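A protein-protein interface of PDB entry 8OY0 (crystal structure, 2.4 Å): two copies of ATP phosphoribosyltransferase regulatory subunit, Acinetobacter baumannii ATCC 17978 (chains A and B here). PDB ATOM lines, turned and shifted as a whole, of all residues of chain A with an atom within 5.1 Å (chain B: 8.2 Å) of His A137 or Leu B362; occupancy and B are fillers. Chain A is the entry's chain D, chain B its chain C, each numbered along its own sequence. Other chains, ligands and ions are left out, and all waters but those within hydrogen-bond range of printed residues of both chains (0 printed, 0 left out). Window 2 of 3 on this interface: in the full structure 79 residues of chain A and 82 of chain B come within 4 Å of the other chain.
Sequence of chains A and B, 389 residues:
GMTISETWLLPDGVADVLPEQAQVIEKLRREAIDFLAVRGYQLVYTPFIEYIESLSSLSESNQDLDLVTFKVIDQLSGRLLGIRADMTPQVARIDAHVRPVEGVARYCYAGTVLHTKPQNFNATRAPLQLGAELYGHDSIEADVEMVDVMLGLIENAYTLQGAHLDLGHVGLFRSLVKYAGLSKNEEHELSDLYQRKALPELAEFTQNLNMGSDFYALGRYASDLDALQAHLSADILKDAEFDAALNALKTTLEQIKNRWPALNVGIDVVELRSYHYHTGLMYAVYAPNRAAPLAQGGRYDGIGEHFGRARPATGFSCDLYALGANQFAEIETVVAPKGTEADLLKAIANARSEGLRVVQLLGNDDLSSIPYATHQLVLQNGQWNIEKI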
ATOM      1  N   VAL A 104       9.130  20.973 -10.701  1.00  0.00           N
ATOM      2  CA  VAL A 104       8.308  22.162 -10.847  1.00  0.00           C
ATOM      3  C   VAL A 104       8.820  23.236  -9.892  1.00  0.00           C
ATOM      4  O   VAL A 104       9.221  22.926  -8.768  1.00  0.00           O
ATOM      5  CB  VAL A 104       6.826  21.834 -10.581  1.00  0.00           C
ATOM      6  CG1 VAL A 104       5.970  23.083 -10.462  1.00  0.00           C
ATOM      7  CG2 VAL A 104       6.258  20.902 -11.644  1.00  0.00           C
ATOM      8  N   ARG A 106       8.071  27.562  -8.677  1.00  0.00           N
ATOM      9  CA  ARG A 106       7.158  28.690  -8.670  1.00  0.00           C
ATOM     10  C   ARG A 106       7.844  29.887  -8.019  1.00  0.00           C
ATOM     11  O   ARG A 106       8.360  29.767  -6.912  1.00  0.00           O
ATOM     12  CB  ARG A 106       5.900  28.327  -7.875  1.00  0.00           C
ATOM     13  CG  ARG A 106       5.043  27.223  -8.483  1.00  0.00           C
ATOM     14  CD  ARG A 106       3.817  26.979  -7.620  1.00  0.00           C
ATOM     15  NE  ARG A 106       2.836  26.068  -8.196  1.00  0.00           N
ATOM     16  CZ  ARG A 106       2.962  24.744  -8.291  1.00  0.00           C
ATOM     17  NH1 ARG A 106       4.029  24.127  -7.817  1.00  0.00           N
ATOM     18  NH2 ARG A 106       2.002  24.033  -8.858  1.00  0.00           N
ATOM     19  N   LEU A 134       5.479  29.906 -13.361  1.00  0.00           N
ATOM     20  CA  LEU A 134       5.397  28.484 -13.061  1.00  0.00           C
ATOM     21  C   LEU A 134       6.209  27.727 -14.109  1.00  0.00           C
ATOM     22  O   LEU A 134       5.851  27.718 -15.284  1.00  0.00           O
ATOM     23  CB  LEU A 134       3.918  28.080 -13.074  1.00  0.00           C
ATOM     24  CG  LEU A 134       3.543  26.745 -12.423  1.00  0.00           C
ATOM     25  CD1 LEU A 134       2.050  26.491 -12.576  1.00  0.00           C
ATOM     26  CD2 LEU A 134       4.320  25.586 -13.011  1.00  0.00           C
ATOM     27  N   TYR A 135       7.312  27.109 -13.670  1.00  0.00           N
ATOM     28  CA  TYR A 135       8.235  26.412 -14.552  1.00  0.00           C
ATOM     29  C   TYR A 135       8.144  24.908 -14.319  1.00  0.00           C
ATOM     30  O   TYR A 135       7.885  24.472 -13.201  1.00  0.00           O
ATOM     31  CB  TYR A 135       9.674  26.860 -14.287  1.00  0.00           C
ATOM     32  CG  TYR A 135       9.923  28.334 -14.471  1.00  0.00           C
ATOM     33  CD1 TYR A 135      10.125  28.873 -15.733  1.00  0.00           C
ATOM     34  CD2 TYR A 135       9.936  29.195 -13.384  1.00  0.00           C
ATOM     35  CE1 TYR A 135      10.346  30.226 -15.911  1.00  0.00           C
ATOM     36  CE2 TYR A 135      10.157  30.552 -13.546  1.00  0.00           C
ATOM     37  CZ  TYR A 135      10.357  31.069 -14.814  1.00  0.00           C
ATOM     38  OH  TYR A 135      10.560  32.418 -14.971  1.00  0.00           O
ATOM     39  N   GLY A 136       8.357  24.126 -15.384  1.00  0.00           N
ATOM     40  CA  GLY A 136       8.648  22.706 -15.250  1.00  0.00           C
ATOM     41  C   GLY A 136       7.435  21.787 -15.399  1.00  0.00           C
ATOM     42  O   GLY A 136       7.552  20.600 -15.114  1.00  0.00           O
ATOM     43  N   HIS A 137       6.284  22.306 -15.850  1.00  0.00           N
ATOM     44  CA  HIS A 137       5.129  21.452 -16.113  1.00  0.00           C
ATOM     45  C   HIS A 137       4.581  21.734 -17.507  1.00  0.00           C
ATOM     46  O   HIS A 137       4.192  22.865 -17.792  1.00  0.00           O
ATOM     47  CB  HIS A 137       4.025  21.639 -15.067  1.00  0.00           C
ATOM     48  CG  HIS A 137       2.908  20.660 -15.234  1.00  0.00           C
ATOM     49  ND1 HIS A 137       2.947  19.389 -14.702  1.00  0.00           N
ATOM     50  CD2 HIS A 137       1.727  20.756 -15.863  1.00  0.00           C
ATOM     51  CE1 HIS A 137       1.829  18.750 -15.013  1.00  0.00           C
ATOM     52  NE2 HIS A 137       1.074  19.562 -15.717  1.00  0.00           N
ATOM     53  N   ASP A 138       4.520  20.691 -18.343  1.00  0.00           N
ATOM     54  CA  ASP A 138       4.160  20.832 -19.748  1.00  0.00           C
ATOM     55  C   ASP A 138       2.662  21.074 -19.925  1.00  0.00           C
ATOM     56  O   ASP A 138       2.281  21.939 -20.706  1.00  0.00           O
ATOM     57  CB  ASP A 138       4.586  19.611 -20.571  1.00  0.00           C
ATOM     58  CG  ASP A 138       6.089  19.521 -20.781  1.00  0.00           C
ATOM     59  OD1 ASP A 138       6.704  20.553 -21.140  1.00  0.00           O
ATOM     60  OD2 ASP A 138       6.629  18.413 -20.613  1.00  0.00           O
ATOM     61  N   SER A 139       1.819  20.316 -19.213  1.00  0.00           N
ATOM     62  CA  SER A 139       0.412  20.195 -19.578  1.00  0.00           C
ATOM     63  C   SER A 139      -0.354  21.486 -19.296  1.00  0.00           C
ATOM     64  O   SER A 139       0.090  22.344 -18.539  1.00  0.00           O
ATOM     65  CB  SER A 139      -0.251  19.027 -18.891  1.00  0.00           C
ATOM     66  OG  SER A 139      -0.771  19.409 -17.627  1.00  0.00           O
ATOM     67  N   GLU A 141      -2.677  22.148 -17.479  1.00  0.00           N
ATOM     68  CA  GLU A 141      -3.071  22.378 -16.096  1.00  0.00           C
ATOM     69  C   GLU A 141      -2.237  23.473 -15.430  1.00  0.00           C
ATOM     70  O   GLU A 141      -2.723  24.141 -14.519  1.00  0.00           O
ATOM     71  CB  GLU A 141      -2.944  21.087 -15.301  1.00  0.00           C
ATOM     72  CG  GLU A 141      -4.079  20.120 -15.567  1.00  0.00           C
ATOM     73  CD  GLU A 141      -4.208  19.102 -14.455  1.00  0.00           C
ATOM     74  OE1 GLU A 141      -4.048  19.522 -13.285  1.00  0.00           O
ATOM     75  OE2 GLU A 141      -4.467  17.908 -14.754  1.00  0.00           O
ATOM     76  N   ALA A 142      -0.979  23.629 -15.860  1.00  0.00           N
ATOM     77  CA  ALA A 142      -0.123  24.685 -15.347  1.00  0.00           C
ATOM     78  C   ALA A 142      -0.716  26.049 -15.700  1.00  0.00           C
ATOM     79  O   ALA A 142      -0.701  26.971 -14.880  1.00  0.00           O
ATOM     80  CB  ALA A 142       1.276  24.522 -15.893  1.00  0.00           C
ATOM     81  N   GLU A 145      -3.834  26.760 -13.545  1.00  0.00           N
ATOM     82  CA  GLU A 145      -3.420  27.269 -12.247  1.00  0.00           C
ATOM     83  C   GLU A 145      -3.099  28.757 -12.372  1.00  0.00           C
ATOM     84  O   GLU A 145      -3.590  29.566 -11.588  1.00  0.00           O
ATOM     85  CB  GLU A 145      -2.206  26.516 -11.696  1.00  0.00           C
ATOM     86  CG  GLU A 145      -1.814  26.966 -10.296  1.00  0.00           C
ATOM     87  CD  GLU A 145      -0.535  26.367  -9.734  1.00  0.00           C
ATOM     88  OE1 GLU A 145      -0.380  25.137  -9.821  1.00  0.00           O
ATOM     89  OE2 GLU A 145       0.287  27.129  -9.180  1.00  0.00           O
ATOM     90  N   ARG A 299       1.529  31.037 -21.850  1.00  0.00           N
ATOM     91  CA  ARG A 299       2.465  29.937 -21.955  1.00  0.00           C
ATOM     92  C   ARG A 299       3.654  30.388 -22.797  1.00  0.00           C
ATOM     93  O   ARG A 299       3.460  30.878 -23.905  1.00  0.00           O
ATOM     94  CB  ARG A 299       1.724  28.759 -22.597  1.00  0.00           C
ATOM     95  CG  ARG A 299       2.610  27.587 -22.991  1.00  0.00           C
ATOM     96  CD  ARG A 299       3.235  26.873 -21.819  1.00  0.00           C
ATOM     97  NE  ARG A 299       2.253  26.194 -20.995  1.00  0.00           N
ATOM     98  CZ  ARG A 299       2.539  25.211 -20.150  1.00  0.00           C
ATOM     99  NH1 ARG A 299       3.785  24.777 -20.022  1.00  0.00           N
ATOM    100  NH2 ARG A 299       1.573  24.641 -19.451  1.00  0.00           N
ATOM    101  N   PRO A 312       9.638  24.260 -19.625  1.00  0.00           N
ATOM    102  CA  PRO A 312       8.252  24.689 -19.788  1.00  0.00           C
ATOM    103  C   PRO A 312       7.999  25.812 -18.780  1.00  0.00           C
ATOM    104  O   PRO A 312       8.538  25.794 -17.675  1.00  0.00           O
ATOM    105  CB  PRO A 312       7.407  23.426 -19.550  1.00  0.00           C
ATOM    106  CG  PRO A 312       8.345  22.442 -18.856  1.00  0.00           C
ATOM    107  CD  PRO A 312       9.761  22.853 -19.215  1.00  0.00           C
ATOM    108  N   VAL B 335       2.933  19.873   0.089  1.00  0.00           N
ATOM    109  CA  VAL B 335       2.422  19.385  -1.181  1.00  0.00           C
ATOM    110  C   VAL B 335       1.125  18.622  -0.935  1.00  0.00           C
ATOM    111  O   VAL B 335       1.103  17.682  -0.147  1.00  0.00           O
ATOM    112  CB  VAL B 335       3.447  18.492  -1.902  1.00  0.00           C
ATOM    113  CG1 VAL B 335       2.904  17.977  -3.227  1.00  0.00           C
ATOM    114  CG2 VAL B 335       4.766  19.213  -2.099  1.00  0.00           C
ATOM    115  N   ALA B 336       0.059  19.042  -1.623  1.00  0.00           N
ATOM    116  CA  ALA B 336      -1.210  18.334  -1.631  1.00  0.00           C
ATOM    117  C   ALA B 336      -1.425  17.718  -3.007  1.00  0.00           C
ATOM    118  O   ALA B 336      -0.813  18.158  -3.977  1.00  0.00           O
ATOM    119  CB  ALA B 336      -2.325  19.287  -1.280  1.00  0.00           C
ATOM    120  N   PRO B 337      -2.288  16.687  -3.148  1.00  0.00           N
ATOM    121  CA  PRO B 337      -2.582  16.117  -4.461  1.00  0.00           C
ATOM    122  C   PRO B 337      -3.451  17.039  -5.309  1.00  0.00           C
ATOM    123  O   PRO B 337      -4.071  17.971  -4.795  1.00  0.00           O
ATOM    124  CB  PRO B 337      -3.320  14.808  -4.141  1.00  0.00           C
ATOM    125  CG  PRO B 337      -3.938  15.051  -2.784  1.00  0.00           C
ATOM    126  CD  PRO B 337      -2.996  15.995  -2.062  1.00  0.00           C
ATOM    127  N   LYS B 338      -3.458  16.774  -6.620  1.00  0.00           N
ATOM    128  CA  LYS B 338      -4.356  17.428  -7.554  1.00  0.00           C
ATOM    129  C   LYS B 338      -5.795  17.140  -7.148  1.00  0.00           C
ATOM    130  O   LYS B 338      -6.083  16.045  -6.674  1.00  0.00           O
ATOM    131  CB  LYS B 338      -4.112  16.899  -8.970  1.00  0.00           C
ATOM    132  CG  LYS B 338      -5.063  17.434 -10.036  1.00  0.00           C
ATOM    133  CD  LYS B 338      -5.023  16.650 -11.321  1.00  0.00           C
ATOM    134  CE  LYS B 338      -6.155  17.011 -12.253  1.00  0.00           C
ATOM    135  NZ  LYS B 338      -6.107  16.191 -13.482  1.00  0.00           N
ATOM    136  N   GLY B 339      -6.683  18.125  -7.346  1.00  0.00           N
ATOM    137  CA  GLY B 339      -8.109  17.920  -7.158  1.00  0.00           C
ATOM    138  C   GLY B 339      -8.845  19.181  -6.705  1.00  0.00           C
ATOM    139  O   GLY B 339      -8.232  20.130  -6.221  1.00  0.00           O
ATOM    140  N   VAL B 359       1.142  23.849  -2.209  1.00  0.00           N
ATOM    141  CA  VAL B 359       0.976  23.658  -3.638  1.00  0.00           C
ATOM    142  C   VAL B 359       0.247  22.339  -3.859  1.00  0.00           C
ATOM    143  O   VAL B 359       0.260  21.473  -2.988  1.00  0.00           O
ATOM    144  CB  VAL B 359       2.323  23.678  -4.382  1.00  0.00           C
ATOM    145  CG1 VAL B 359       2.994  25.037  -4.280  1.00  0.00           C
ATOM    146  CG2 VAL B 359       3.270  22.585  -3.907  1.00  0.00           C
ATOM    147  N   GLN B 360      -0.399  22.226  -5.023  1.00  0.00           N
ATOM    148  CA  GLN B 360      -1.009  20.989  -5.470  1.00  0.00           C
ATOM    149  C   GLN B 360      -0.185  20.424  -6.624  1.00  0.00           C
ATOM    150  O   GLN B 360       0.345  21.169  -7.445  1.00  0.00           O
ATOM    151  CB  GLN B 360      -2.454  21.233  -5.909  1.00  0.00           C
ATOM    152  CG  GLN B 360      -3.428  21.358  -4.747  1.00  0.00           C
ATOM    153  CD  GLN B 360      -4.862  21.509  -5.196  1.00  0.00           C
ATOM    154  OE1 GLN B 360      -5.311  22.597  -5.542  1.00  0.00           O
ATOM    155  NE2 GLN B 360      -5.609  20.421  -5.158  1.00  0.00           N
ATOM    156  N   LEU B 361      -0.091  19.094  -6.673  1.00  0.00           N
ATOM    157  CA  LEU B 361       0.512  18.404  -7.800  1.00  0.00           C
ATOM    158  C   LEU B 361      -0.273  18.746  -9.063  1.00  0.00           C
ATOM    159  O   LEU B 361      -1.490  18.921  -9.026  1.00  0.00           O
ATOM    160  CB  LEU B 361       0.504  16.894  -7.537  1.00  0.00           C
ATOM    161  CG  LEU B 361       1.335  16.418  -6.347  1.00  0.00           C
ATOM    162  CD1 LEU B 361       1.347  14.899  -6.264  1.00  0.00           C
ATOM    163  CD2 LEU B 361       2.750  16.968  -6.420  1.00  0.00           C
ATOM    164  N   LEU B 362       0.452  18.852 -10.182  1.00  0.00           N
ATOM    165  CA  LEU B 362      -0.126  19.174 -11.476  1.00  0.00           C
ATOM    166  C   LEU B 362      -0.227  17.910 -12.328  1.00  0.00           C
ATOM    167  O   LEU B 362       0.728  17.151 -12.421  1.00  0.00           O
ATOM    168  CB  LEU B 362       0.759  20.234 -12.146  1.00  0.00           C
ATOM    169  CG  LEU B 362       0.659  21.634 -11.535  1.00  0.00           C
ATOM    170  CD1 LEU B 362       1.813  22.509 -11.995  1.00  0.00           C
ATOM    171  CD2 LEU B 362      -0.675  22.289 -11.877  1.00  0.00           C
ATOM    172  N   GLY B 363      -1.392  17.698 -12.946  1.00  0.00           N
ATOM    173  CA  GLY B 363      -1.595  16.594 -13.869  1.00  0.00           C
ATOM    174  C   GLY B 363      -1.212  15.255 -13.247  1.00  0.00           C
ATOM    175  O   GLY B 363      -1.731  14.896 -12.195  1.00  0.00           O
ATOM    176  N   ASN B 364      -0.272  14.548 -13.890  1.00  0.00           N
ATOM    177  CA  ASN B 364       0.147  13.220 -13.469  1.00  0.00           C
ATOM    178  C   ASN B 364       1.441  13.276 -12.658  1.00  0.00           C
ATOM    179  O   ASN B 364       2.039  12.236 -12.398  1.00  0.00           O
ATOM    180  CB  ASN B 364       0.343  12.301 -14.675  1.00  0.00           C
ATOM    181  CG  ASN B 364      -0.932  12.060 -15.458  1.00  0.00           C
ATOM    182  OD1 ASN B 364      -2.027  12.387 -14.997  1.00  0.00           O
ATOM    183  ND2 ASN B 364      -0.804  11.475 -16.637  1.00  0.00           N
ATOM    184  N   ASP B 365       1.875  14.484 -12.264  1.00  0.00           N
ATOM    185  CA  ASP B 365       3.080  14.650 -11.467  1.00  0.00           C
ATOM    186  C   ASP B 365       2.909  13.930 -10.128  1.00  0.00           C
ATOM    187  O   ASP B 365       1.847  13.994  -9.512  1.00  0.00           O
ATOM    188  CB  ASP B 365       3.399  16.129 -11.206  1.00  0.00           C
ATOM    189  CG  ASP B 365       3.805  16.960 -12.420  1.00  0.00           C
ATOM    190  OD1 ASP B 365       3.924  16.390 -13.526  1.00  0.00           O
ATOM    191  OD2 ASP B 365       3.973  18.193 -12.254  1.00  0.00           O
ATOM    192  N   ASP B 366       3.970  13.251  -9.675  1.00  0.00           N
ATOM    193  CA  ASP B 366       4.026  12.720  -8.321  1.00  0.00           C
ATOM    194  C   ASP B 366       4.808  13.702  -7.448  1.00  0.00           C
ATOM    195  O   ASP B 366       5.168  14.785  -7.894  1.00  0.00           O
ATOM    196  CB  ASP B 366       4.572  11.284  -8.298  1.00  0.00           C
ATOM    197  CG  ASP B 366       5.975  11.109  -8.856  1.00  0.00           C
ATOM    198  OD1 ASP B 366       6.840  11.950  -8.552  1.00  0.00           O
ATOM    199  OD2 ASP B 366       6.199  10.112  -9.572  1.00  0.00           O
ATOM    200  N   SER B 369       8.123  15.722  -8.230  1.00  0.00           N
ATOM    201  CA  SER B 369       8.063  16.953  -9.007  1.00  0.00           C
ATOM    202  C   SER B 369       8.333  18.177  -8.129  1.00  0.00           C
ATOM    203  O   SER B 369       8.678  19.237  -8.644  1.00  0.00           O
ATOM    204  CB  SER B 369       6.736  17.088  -9.728  1.00  0.00           C
ATOM    205  OG  SER B 369       5.669  17.269  -8.811  1.00  0.00           O
ATOM    206  N   ILE B 370       8.143  18.029  -6.811  1.00  0.00           N
ATOM    207  CA  ILE B 370       8.453  19.076  -5.848  1.00  0.00           C
ATOM    208  C   ILE B 370       9.569  18.572  -4.925  1.00  0.00           C
ATOM    209  O   ILE B 370       9.315  18.220  -3.777  1.00  0.00           O
ATOM    210  CB  ILE B 370       7.188  19.473  -5.057  1.00  0.00           C
ATOM    211  CG1 ILE B 370       5.957  19.654  -5.955  1.00  0.00           C
ATOM    212  CG2 ILE B 370       7.445  20.700  -4.206  1.00  0.00           C
ATOM    213  CD1 ILE B 370       6.034  20.846  -6.890  1.00  0.00           C
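The side-chain amino group (NZ) of Lys B338 is in salt-bridge range of the side-chain carboxylate (OE2) of Glu A141 (2.7 Å).
The side-chain carboxylate (OE1) of Glu A141 lies within hydrogen-bond range of the backbone NH (N) of Gly B363 (3.2 Å).
A ring nitrogen (ND1) of His A137 sits at hydrogen-bond distance from the side-chain carboxylate of Asp B365 (2.9 Å).
The backbone carbonyl oxygen of Ser B369 lies within hydrogen-bond range of the backbone NH of Val A104 (2.7 Å).
The backbone carbonyl oxygen (O) of Val B359 sits at hydrogen-bond distance from the backbone NH (N) of Ala B336.
The backbone carbonyl oxygen (O) of Pro B337 lies within hydrogen-bond range of the side-chain amide nitrogen (NE2) of Gln B360.
O of Gly B339 sits at hydrogen-bond distance from NE2 of Gln B360.
The side-chain hydroxyl (OG) of Ser B369 sits at hydrogen-bond distance from the backbone carbonyl oxygen (O) of Asp B366 (2.7 Å).
The side-chain hydroxyl (OG) of Ser A139 is in hydrogen-bond range of a ring nitrogen (NE2) of His A137, 2.7 Å away.
O of His A137 is in hydrogen-bond range of NH1 of Arg A299 (3.0 Å).
Among the printed residues, merely in contact across the chains: Val A104 with Asp B365 (3.6 Å), Val A104 with Ile B370 (3.9 Å), Arg A106 with Val B359 (3.8 Å), Arg A106 with Gln B360 (3.6 Å), Arg A106 with Leu B362 (3.5 Å), Arg A106 with Ile B370 (3.96 Å), His A137 with Leu B362 (3.2 Å), His A137 with Gly B363 (3.97 Å), Glu A141 with Leu B362 (3.8 Å) and Glu A145 with Leu B362 (3.5 Å).
Of the printed residues of chain B, Arg A106 touches Val B359 (3.8 Å), Gln B360 (3.6 Å), Leu B362 (3.5 Å) and Ile B370 (3.96 Å).
No residue of chain B comes within 4 Å of Gly A136.
Of chain B, only Leu B362, Gly B363 and Asp B365 come within 4 Å of His A137.
Asp A138 touches none of the printed residues of chain B.
No residue of chain B comes within 4 Å of Ser A139.
Of the printed residues of chain A, Ser B369 touches Val A104 (2.7 Å).
The nearest printed residue of chain B that does not touch Val A104 is Leu B362 (4.5 Å).
Hydrophobic or aromatic side chains of chain B that line the printed part of chain A: Val B359, Leu B362 and Ile B370.
Of the 13 printed residues of chain A, 5 touch a printed residue of chain B.
Hydrophobic or aromatic side chains of chain A within 4 Å of the printed part of chain B: Val A104 and His A137.
Among the printed residues, Asp or Glu carboxylates within 4 Å of a Lys or Arg side-chain nitrogen of the other chain: Glu A141 with Lys B338.
No position is printed for both chains.
Of the 14 pairs that touch across the chains among the printed residues, none has its exchanged pair printed and touching as well.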
